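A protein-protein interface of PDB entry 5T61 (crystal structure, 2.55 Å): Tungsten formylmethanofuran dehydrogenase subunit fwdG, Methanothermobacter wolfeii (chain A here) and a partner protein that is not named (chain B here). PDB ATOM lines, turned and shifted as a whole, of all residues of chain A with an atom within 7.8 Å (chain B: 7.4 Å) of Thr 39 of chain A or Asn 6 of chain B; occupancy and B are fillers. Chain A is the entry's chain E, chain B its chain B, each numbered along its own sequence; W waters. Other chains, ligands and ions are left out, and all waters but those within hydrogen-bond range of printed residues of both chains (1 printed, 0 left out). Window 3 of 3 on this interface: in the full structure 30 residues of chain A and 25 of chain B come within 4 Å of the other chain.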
ATOM      1  N   SER A  29      17.576 -38.532  12.930  1.00  0.00           N
ATOM      2  CA  SER A  29      16.808 -37.376  13.394  1.00  0.00           C
ATOM      3  C   SER A  29      15.842 -36.939  12.303  1.00  0.00           C
ATOM      4  O   SER A  29      16.283 -36.362  11.286  1.00  0.00           O
ATOM      5  CB  SER A  29      17.734 -36.227  13.783  1.00  0.00           C
ATOM      6  OG  SER A  29      16.990 -35.053  14.063  1.00  0.00           O
ATOM      7  N   GLU A  31      13.893 -34.462  12.310  1.00  0.00           N
ATOM      8  CA  GLU A  31      13.957 -33.011  12.170  1.00  0.00           C
ATOM      9  C   GLU A  31      15.081 -32.629  11.217  1.00  0.00           C
ATOM     10  O   GLU A  31      14.926 -31.731  10.379  1.00  0.00           O
ATOM     11  CB  GLU A  31      14.191 -32.374  13.535  1.00  0.00           C
ATOM     12  CG  GLU A  31      13.385 -32.999  14.658  1.00  0.00           C
ATOM     13  CD  GLU A  31      13.786 -32.458  16.011  1.00  0.00           C
ATOM     14  OE1 GLU A  31      14.983 -32.564  16.350  1.00  0.00           O
ATOM     15  OE2 GLU A  31      12.902 -32.005  16.766  1.00  0.00           O
ATOM     16  N   VAL A  32      16.224 -33.308  11.337  1.00  0.00           N
ATOM     17  CA  VAL A  32      17.343 -33.093  10.427  1.00  0.00           C
ATOM     18  C   VAL A  32      16.987 -33.572   9.027  1.00  0.00           C
ATOM     19  O   VAL A  32      17.317 -32.918   8.029  1.00  0.00           O
ATOM     20  CB  VAL A  32      18.607 -33.792  10.963  1.00  0.00           C
ATOM     21  CG1 VAL A  32      19.686 -33.861   9.887  1.00  0.00           C
ATOM     22  CG2 VAL A  32      19.135 -33.059  12.188  1.00  0.00           C
ATOM     23  N   LYS A  36      15.589 -29.222   9.548  1.00  0.00           N
ATOM     24  CA  LYS A  36      15.714 -28.438  10.768  1.00  0.00           C
ATOM     25  C   LYS A  36      16.937 -28.871  11.563  1.00  0.00           C
ATOM     26  O   LYS A  36      17.393 -30.011  11.468  1.00  0.00           O
ATOM     27  CB  LYS A  36      14.467 -28.582  11.636  1.00  0.00           C
ATOM     28  CG  LYS A  36      13.205 -28.062  10.992  1.00  0.00           C
ATOM     29  CD  LYS A  36      12.010 -28.731  11.631  1.00  0.00           C
ATOM     30  CE  LYS A  36      10.725 -28.013  11.294  1.00  0.00           C
ATOM     31  NZ  LYS A  36       9.627 -28.503  12.169  1.00  0.00           N
ATOM     32  N   GLY A  37      17.465 -27.944  12.358  1.00  0.00           N
ATOM     33  CA  GLY A  37      18.425 -28.302  13.372  1.00  0.00           C
ATOM     34  C   GLY A  37      17.753 -29.159  14.420  1.00  0.00           C
ATOM     35  O   GLY A  37      16.554 -29.022  14.686  1.00  0.00           O
ATOM     36  N   PRO A  38      18.503 -30.077  15.029  1.00  0.00           N
ATOM     37  CA  PRO A  38      17.906 -30.945  16.051  1.00  0.00           C
ATOM     38  C   PRO A  38      17.511 -30.150  17.289  1.00  0.00           C
ATOM     39  O   PRO A  38      18.269 -29.305  17.771  1.00  0.00           O
ATOM     40  CB  PRO A  38      19.016 -31.959  16.356  1.00  0.00           C
ATOM     41  CG  PRO A  38      20.278 -31.297  15.913  1.00  0.00           C
ATOM     42  CD  PRO A  38      19.915 -30.403  14.767  1.00  0.00           C
ATOM     43  N   THR A  39      16.299 -30.410  17.779  1.00  0.00           N
ATOM     44  CA  THR A  39      15.849 -29.945  19.087  1.00  0.00           C
ATOM     45  C   THR A  39      15.825 -31.076  20.106  1.00  0.00           C
ATOM     46  O   THR A  39      16.341 -30.925  21.217  1.00  0.00           O
ATOM     47  CB  THR A  39      14.455 -29.309  18.986  1.00  0.00           C
ATOM     48  OG1 THR A  39      14.489 -28.200  18.080  1.00  0.00           O
ATOM     49  CG2 THR A  39      13.974 -28.846  20.351  1.00  0.00           C
ATOM     50  N   ASP A  40      15.246 -32.215  19.738  1.00  0.00           N
ATOM     51  CA  ASP A  40      15.395 -33.421  20.534  1.00  0.00           C
ATOM     52  C   ASP A  40      16.870 -33.781  20.675  1.00  0.00           C
ATOM     53  O   ASP A  40      17.688 -33.514  19.792  1.00  0.00           O
ATOM     54  CB  ASP A  40      14.632 -34.585  19.896  1.00  0.00           C
ATOM     55  CG  ASP A  40      13.129 -34.354  19.861  1.00  0.00           C
ATOM     56  OD1 ASP A  40      12.635 -33.493  20.622  1.00  0.00           O
ATOM     57  OD2 ASP A  40      12.444 -35.028  19.064  1.00  0.00           O
ATOM     58  N   ASP A  41      17.204 -34.392  21.806  1.00  0.00           N
ATOM     59  CA  ASP A  41      18.549 -34.902  22.034  1.00  0.00           C
ATOM     60  C   ASP A  41      18.805 -36.089  21.111  1.00  0.00           C
ATOM     61  O   ASP A  41      18.048 -37.063  21.130  1.00  0.00           O
ATOM     62  CB  ASP A  41      18.694 -35.320  23.494  1.00  0.00           C
ATOM     63  CG  ASP A  41      18.558 -34.155  24.457  1.00  0.00           C
ATOM     64  OD1 ASP A  41      18.730 -32.996  24.023  1.00  0.00           O
ATOM     65  OD2 ASP A  41      18.223 -34.400  25.636  1.00  0.00           O
ATOM     66  N   VAL A  42      19.869 -36.017  20.308  1.00  0.00           N
ATOM     67  CA  VAL A  42      20.230 -37.094  19.392  1.00  0.00           C
ATOM     68  C   VAL A  42      21.747 -37.174  19.281  1.00  0.00           C
ATOM     69  O   VAL A  42      22.460 -36.185  19.484  1.00  0.00           O
ATOM     70  CB  VAL A  42      19.599 -36.927  17.984  1.00  0.00           C
ATOM     71  CG1 VAL A  42      18.112 -37.270  17.998  1.00  0.00           C
ATOM     72  CG2 VAL A  42      19.821 -35.516  17.458  1.00  0.00           C
ATOM     73  N   VAL B   4      18.082 -23.345  26.436  1.00  0.00           N
ATOM     74  CA  VAL B   4      16.723 -22.910  26.135  1.00  0.00           C
ATOM     75  C   VAL B   4      16.454 -23.224  24.672  1.00  0.00           C
ATOM     76  O   VAL B   4      17.171 -22.756  23.780  1.00  0.00           O
ATOM     77  CB  VAL B   4      16.519 -21.418  26.436  1.00  0.00           C
ATOM     78  CG1 VAL B   4      15.115 -20.993  26.041  1.00  0.00           C
ATOM     79  CG2 VAL B   4      16.761 -21.135  27.914  1.00  0.00           C
ATOM     80  N   LYS B   5      15.416 -24.008  24.423  1.00  0.00           N
ATOM     81  CA  LYS B   5      15.146 -24.537  23.098  1.00  0.00           C
ATOM     82  C   LYS B   5      14.038 -23.742  22.415  1.00  0.00           C
ATOM     83  O   LYS B   5      13.383 -22.887  23.013  1.00  0.00           O
ATOM     84  CB  LYS B   5      14.764 -26.017  23.196  1.00  0.00           C
ATOM     85  CG  LYS B   5      15.847 -26.880  23.833  1.00  0.00           C
ATOM     86  CD  LYS B   5      15.451 -28.350  23.869  1.00  0.00           C
ATOM     87  CE  LYS B   5      16.639 -29.220  24.257  1.00  0.00           C
ATOM     88  NZ  LYS B   5      16.289 -30.666  24.357  1.00  0.00           N
ATOM     89  N   ASN B   6      13.855 -24.032  21.126  1.00  0.00           N
ATOM     90  CA  ASN B   6      12.786 -23.456  20.307  1.00  0.00           C
ATOM     91  C   ASN B   6      12.864 -21.932  20.231  1.00  0.00           C
ATOM     92  O   ASN B   6      11.855 -21.264  19.999  1.00  0.00           O
ATOM     93  CB  ASN B   6      11.413 -23.902  20.823  1.00  0.00           C
ATOM     94  CG  ASN B   6      11.243 -25.412  20.801  1.00  0.00           C
ATOM     95  OD1 ASN B   6      11.526 -26.063  19.797  1.00  0.00           O
ATOM     96  ND2 ASN B   6      10.797 -25.978  21.916  1.00  0.00           N
ATOM     97  N   VAL B   7      14.065 -21.371  20.374  1.00  0.00           N
ATOM     98  CA  VAL B   7      14.260 -19.926  20.312  1.00  0.00           C
ATOM     99  C   VAL B   7      14.180 -19.462  18.860  1.00  0.00           C
ATOM    100  O   VAL B   7      14.590 -20.177  17.938  1.00  0.00           O
ATOM    101  CB  VAL B   7      15.609 -19.551  20.965  1.00  0.00           C
ATOM    102  CG1 VAL B   7      15.949 -18.079  20.755  1.00  0.00           C
ATOM    103  CG2 VAL B   7      15.594 -19.895  22.446  1.00  0.00           C
ATOM    104  N   VAL B   8      13.649 -18.255  18.647  1.00  0.00           N
ATOM    105  CA  VAL B   8      13.497 -17.672  17.313  1.00  0.00           C
ATOM    106  C   VAL B   8      14.633 -16.681  17.083  1.00  0.00           C
ATOM    107  O   VAL B   8      14.901 -15.826  17.936  1.00  0.00           O
ATOM    108  CB  VAL B   8      12.132 -16.980  17.162  1.00  0.00           C
ATOM    109  CG1 VAL B   8      11.875 -16.626  15.711  1.00  0.00           C
ATOM    110  CG2 VAL B   8      11.014 -17.844  17.735  1.00  0.00           C
ATOM    111  N   CYS B   9      15.308 -16.787  15.933  1.00  0.00           N
ATOM    112  CA  CYS B   9      16.509 -15.958  15.799  1.00  0.00           C
ATOM    113  C   CYS B   9      16.170 -14.580  15.241  1.00  0.00           C
ATOM    114  O   CYS B   9      15.449 -14.479  14.240  1.00  0.00           O
ATOM    115  CB  CYS B   9      17.555 -16.614  14.919  1.00  0.00           C
ATOM    116  SG  CYS B   9      19.043 -15.575  14.818  1.00  0.00           S
ATOM    117  N   CYS B  16      14.470 -18.454  11.573  1.00  0.00           N
ATOM    118  CA  CYS B  16      14.553 -19.788  12.154  1.00  0.00           C
ATOM    119  C   CYS B  16      14.087 -19.773  13.603  1.00  0.00           C
ATOM    120  O   CYS B  16      14.434 -18.878  14.379  1.00  0.00           O
ATOM    121  CB  CYS B  16      15.976 -20.338  12.067  1.00  0.00           C
ATOM    122  SG  CYS B  16      16.419 -20.962  10.434  1.00  0.00           S
ATOM    123  N   ASP B  17      13.286 -20.777  13.963  1.00  0.00           N
ATOM    124  CA  ASP B  17      12.717 -20.878  15.301  1.00  0.00           C
ATOM    125  C   ASP B  17      13.126 -22.165  16.006  1.00  0.00           C
ATOM    126  O   ASP B  17      12.415 -22.623  16.906  1.00  0.00           O
ATOM    127  CB  ASP B  17      11.192 -20.765  15.248  1.00  0.00           C
ATOM    128  CG  ASP B  17      10.538 -21.964  14.584  1.00  0.00           C
ATOM    129  OD1 ASP B  17      10.973 -22.344  13.474  1.00  0.00           O
ATOM    130  OD2 ASP B  17       9.590 -22.529  15.174  1.00  0.00           O
ATOM    131  N   ASP B  18      14.260 -22.760  15.621  1.00  0.00           N
ATOM    132  CA  ASP B  18      14.756 -23.971  16.265  1.00  0.00           C
ATOM    133  C   ASP B  18      16.093 -23.729  16.957  1.00  0.00           C
ATOM    134  O   ASP B  18      16.842 -24.680  17.209  1.00  0.00           O
ATOM    135  CB  ASP B  18      14.891 -25.116  15.256  1.00  0.00           C
ATOM    136  CG  ASP B  18      15.942 -24.843  14.180  1.00  0.00           C
ATOM    137  OD1 ASP B  18      16.387 -23.684  14.030  1.00  0.00           O
ATOM    138  OD2 ASP B  18      16.331 -25.805  13.482  1.00  0.00           O
ATOM    139  N   ILE B  19      16.399 -22.468  17.271  1.00  0.00           N
ATOM    140  CA  ILE B  19      17.672 -22.131  17.891  1.00  0.00           C
ATOM    141  C   ILE B  19      17.690 -22.616  19.331  1.00  0.00           C
ATOM    142  O   ILE B  19      16.709 -22.473  20.072  1.00  0.00           O
ATOM    143  CB  ILE B  19      17.924 -20.616  17.820  1.00  0.00           C
ATOM    144  CG1 ILE B  19      17.814 -20.117  16.378  1.00  0.00           C
ATOM    145  CG2 ILE B  19      19.273 -20.263  18.434  1.00  0.00           C
ATOM    146  CD1 ILE B  19      18.609 -20.927  15.382  1.00  0.00           C
ATOM    147  N   ILE B  20      18.808 -23.204  19.731  1.00  0.00           N
ATOM    148  CA  ILE B  20      19.086 -23.497  21.127  1.00  0.00           C
ATOM    149  C   ILE B  20      20.034 -22.423  21.640  1.00  0.00           C
ATOM    150  O   ILE B  20      21.069 -22.149  21.019  1.00  0.00           O
ATOM    151  CB  ILE B  20      19.684 -24.902  21.279  1.00  0.00           C
ATOM    152  CG1 ILE B  20      18.835 -25.909  20.492  1.00  0.00           C
ATOM    153  CG2 ILE B  20      19.783 -25.280  22.752  1.00  0.00           C
ATOM    154  CD1 ILE B  20      18.508 -27.182  21.220  1.00  0.00           C
ATOM    155  N   CYS B  21      19.667 -21.786  22.745  1.00  0.00           N
ATOM    156  CA  CYS B  21      20.519 -20.801  23.393  1.00  0.00           C
ATOM    157  C   CYS B  21      21.205 -21.432  24.594  1.00  0.00           C
ATOM    158  O   CYS B  21      20.560 -22.112  25.401  1.00  0.00           O
ATOM    159  CB  CYS B  21      19.715 -19.576  23.835  1.00  0.00           C
ATOM    160  SG  CYS B  21      19.240 -18.442  22.514  1.00  0.00           S
ATOM    161  N   ASN B  33      22.624 -24.715  16.305  1.00  0.00           N
ATOM    162  CA  ASN B  33      21.809 -24.686  15.087  1.00  0.00           C
ATOM    163  C   ASN B  33      21.816 -23.334  14.384  1.00  0.00           C
ATOM    164  O   ASN B  33      21.632 -23.273  13.164  1.00  0.00           O
ATOM    165  CB  ASN B  33      20.364 -25.103  15.383  1.00  0.00           C
ATOM    166  CG  ASN B  33      20.265 -26.519  15.900  1.00  0.00           C
ATOM    167  OD1 ASN B  33      21.063 -27.381  15.535  1.00  0.00           O
ATOM    168  ND2 ASN B  33      19.296 -26.761  16.773  1.00  0.00           N
ATOM    169  N   ILE B 401       5.612 -15.496  13.922  1.00  0.00           N
ATOM    170  CA  ILE B 401       6.212 -16.281  14.995  1.00  0.00           C
ATOM    171  C   ILE B 401       6.611 -15.338  16.119  1.00  0.00           C
ATOM    172  O   ILE B 401       7.167 -14.261  15.873  1.00  0.00           O
ATOM    173  CB  ILE B 401       7.432 -17.091  14.504  1.00  0.00           C
ATOM    174  CG1 ILE B 401       7.072 -17.928  13.272  1.00  0.00           C
ATOM    175  CG2 ILE B 401       7.977 -17.972  15.618  1.00  0.00           C
ATOM    176  CD1 ILE B 401       8.273 -18.480  12.528  1.00  0.00           C
ATOM    177  N   ARG B 402       6.341 -15.750  17.353  1.00  0.00           N
ATOM    178  CA  ARG B 402       6.574 -14.890  18.504  1.00  0.00           C
ATOM    179  C   ARG B 402       8.026 -14.983  18.949  1.00  0.00           C
ATOM    180  O   ARG B 402       8.525 -16.076  19.245  1.00  0.00           O
ATOM    181  CB  ARG B 402       5.661 -15.277  19.659  1.00  0.00           C
ATOM    182  CG  ARG B 402       5.801 -14.323  20.813  1.00  0.00           C
ATOM    183  CD  ARG B 402       4.802 -14.591  21.905  1.00  0.00           C
ATOM    184  NE  ARG B 402       4.877 -13.528  22.897  1.00  0.00           N
ATOM    185  CZ  ARG B 402       4.163 -12.412  22.808  1.00  0.00           C
ATOM    186  NH1 ARG B 402       3.341 -12.244  21.779  1.00  0.00           N
ATOM    187  NH2 ARG B 402       4.267 -11.465  23.730  1.00  0.00           N
ATOM    188  N   LYS B 404      11.031 -14.761  21.536  1.00  0.00           N
ATOM    189  CA  LYS B 404      11.096 -15.173  22.929  1.00  0.00           C
ATOM    190  C   LYS B 404      12.045 -14.286  23.726  1.00  0.00           C
ATOM    191  O   LYS B 404      12.995 -13.716  23.185  1.00  0.00           O
ATOM    192  CB  LYS B 404      11.560 -16.625  23.055  1.00  0.00           C
ATOM    193  CG  LYS B 404      10.643 -17.673  22.449  1.00  0.00           C
ATOM    194  CD  LYS B 404      11.085 -19.050  22.934  1.00  0.00           C
ATOM    195  CE  LYS B 404      10.283 -20.180  22.315  1.00  0.00           C
ATOM    196  NZ  LYS B 404       8.936 -20.348  22.922  1.00  0.00           N
HETATM  197  O   HOH W   1      15.472 -25.703  19.521  1.00  0.00           O
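The backbone carbonyl oxygen (O) of Thr 39 of chain A is in hydrogen-bond range of the side-chain amino group (NZ) of Lys 5 of chain B. NZ of Lys 5 of chain B lies within salt-bridge range of OD1 of Asp 41 of chain A, 3.4 Å away. The side-chain carboxylate (OD2) of Asp 18 of chain B is in hydrogen-bond range of the backbone NH (N) of Gly 37 of chain A, at 2.7 Å. The side-chain amide nitrogen (ND2) of Asn 33 of chain B is in hydrogen-bond range of the backbone carbonyl oxygen (O) of Pro 38 of chain A (2.9 Å).
The backbone carbonyl oxygen (O) of Ile 19 of chain B lies within hydrogen-bond range of the backbone NH (N) of Asn 6 of chain B (3.4 Å). The backbone carbonyl oxygen (O) of Val 7 of chain B sits at hydrogen-bond distance from the backbone NH (N) of Asp 18 of chain B (3.5 Å). O of Asp 18 of chain B is in hydrogen-bond range of ND2 of Asn 33 of chain B (3.2 Å). The backbone carbonyl oxygen of Glu 31 of chain A lies within hydrogen-bond range of the backbone NH of Lys 36 of chain A (2.7 Å). OE1 of Glu 31 of chain A lies within hydrogen-bond range of N of Thr 39 of chain A (2.9 Å).
Among the printed residues, merely in contact across the chains: Lys 36 of chain A with Asp 18 of chain B, Gly 37 of chain A with Asn 33 of chain B and Thr 39 of chain A with Asn 6 of chain B.
Of chain B, only Lys 5 (3.2 Å) and Asn 6 (3.7 Å) come within 4 Å of Thr 39 of chain A. Asn 6 of chain B touches just one residue of chain A: Thr 39. Of the printed residues of chain B, Asp 41 of chain A touches Lys 5. Of the printed residues of chain A, Asn 33 of chain B touches Gly 37 (3.5 Å) and Pro 38 (2.9 Å). Of the printed residues of chain A, Asp 18 of chain B touches Lys 36 and Gly 37. The nearest printed residue of chain A that does not touch Asn 33 of chain B is Thr 39 of chain A (4.8 Å).
Of the 16 printed residues of chain B, 4 touch a printed residue of chain A. Printed residues of chain B that touch a printed residue of chain A: Lys 5, Asn 6, Asp 18 and Asn 33. Along chain B the printed residues that touch a printed residue of chain A span positions 5 to 33.
Water W1 lies within hydrogen-bond range of N of Asn 6 of chain B (2.8 Å), O of Asp 18 of chain B (2.9 Å) and OG1 of Thr 39 of chain A (3.0 Å).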
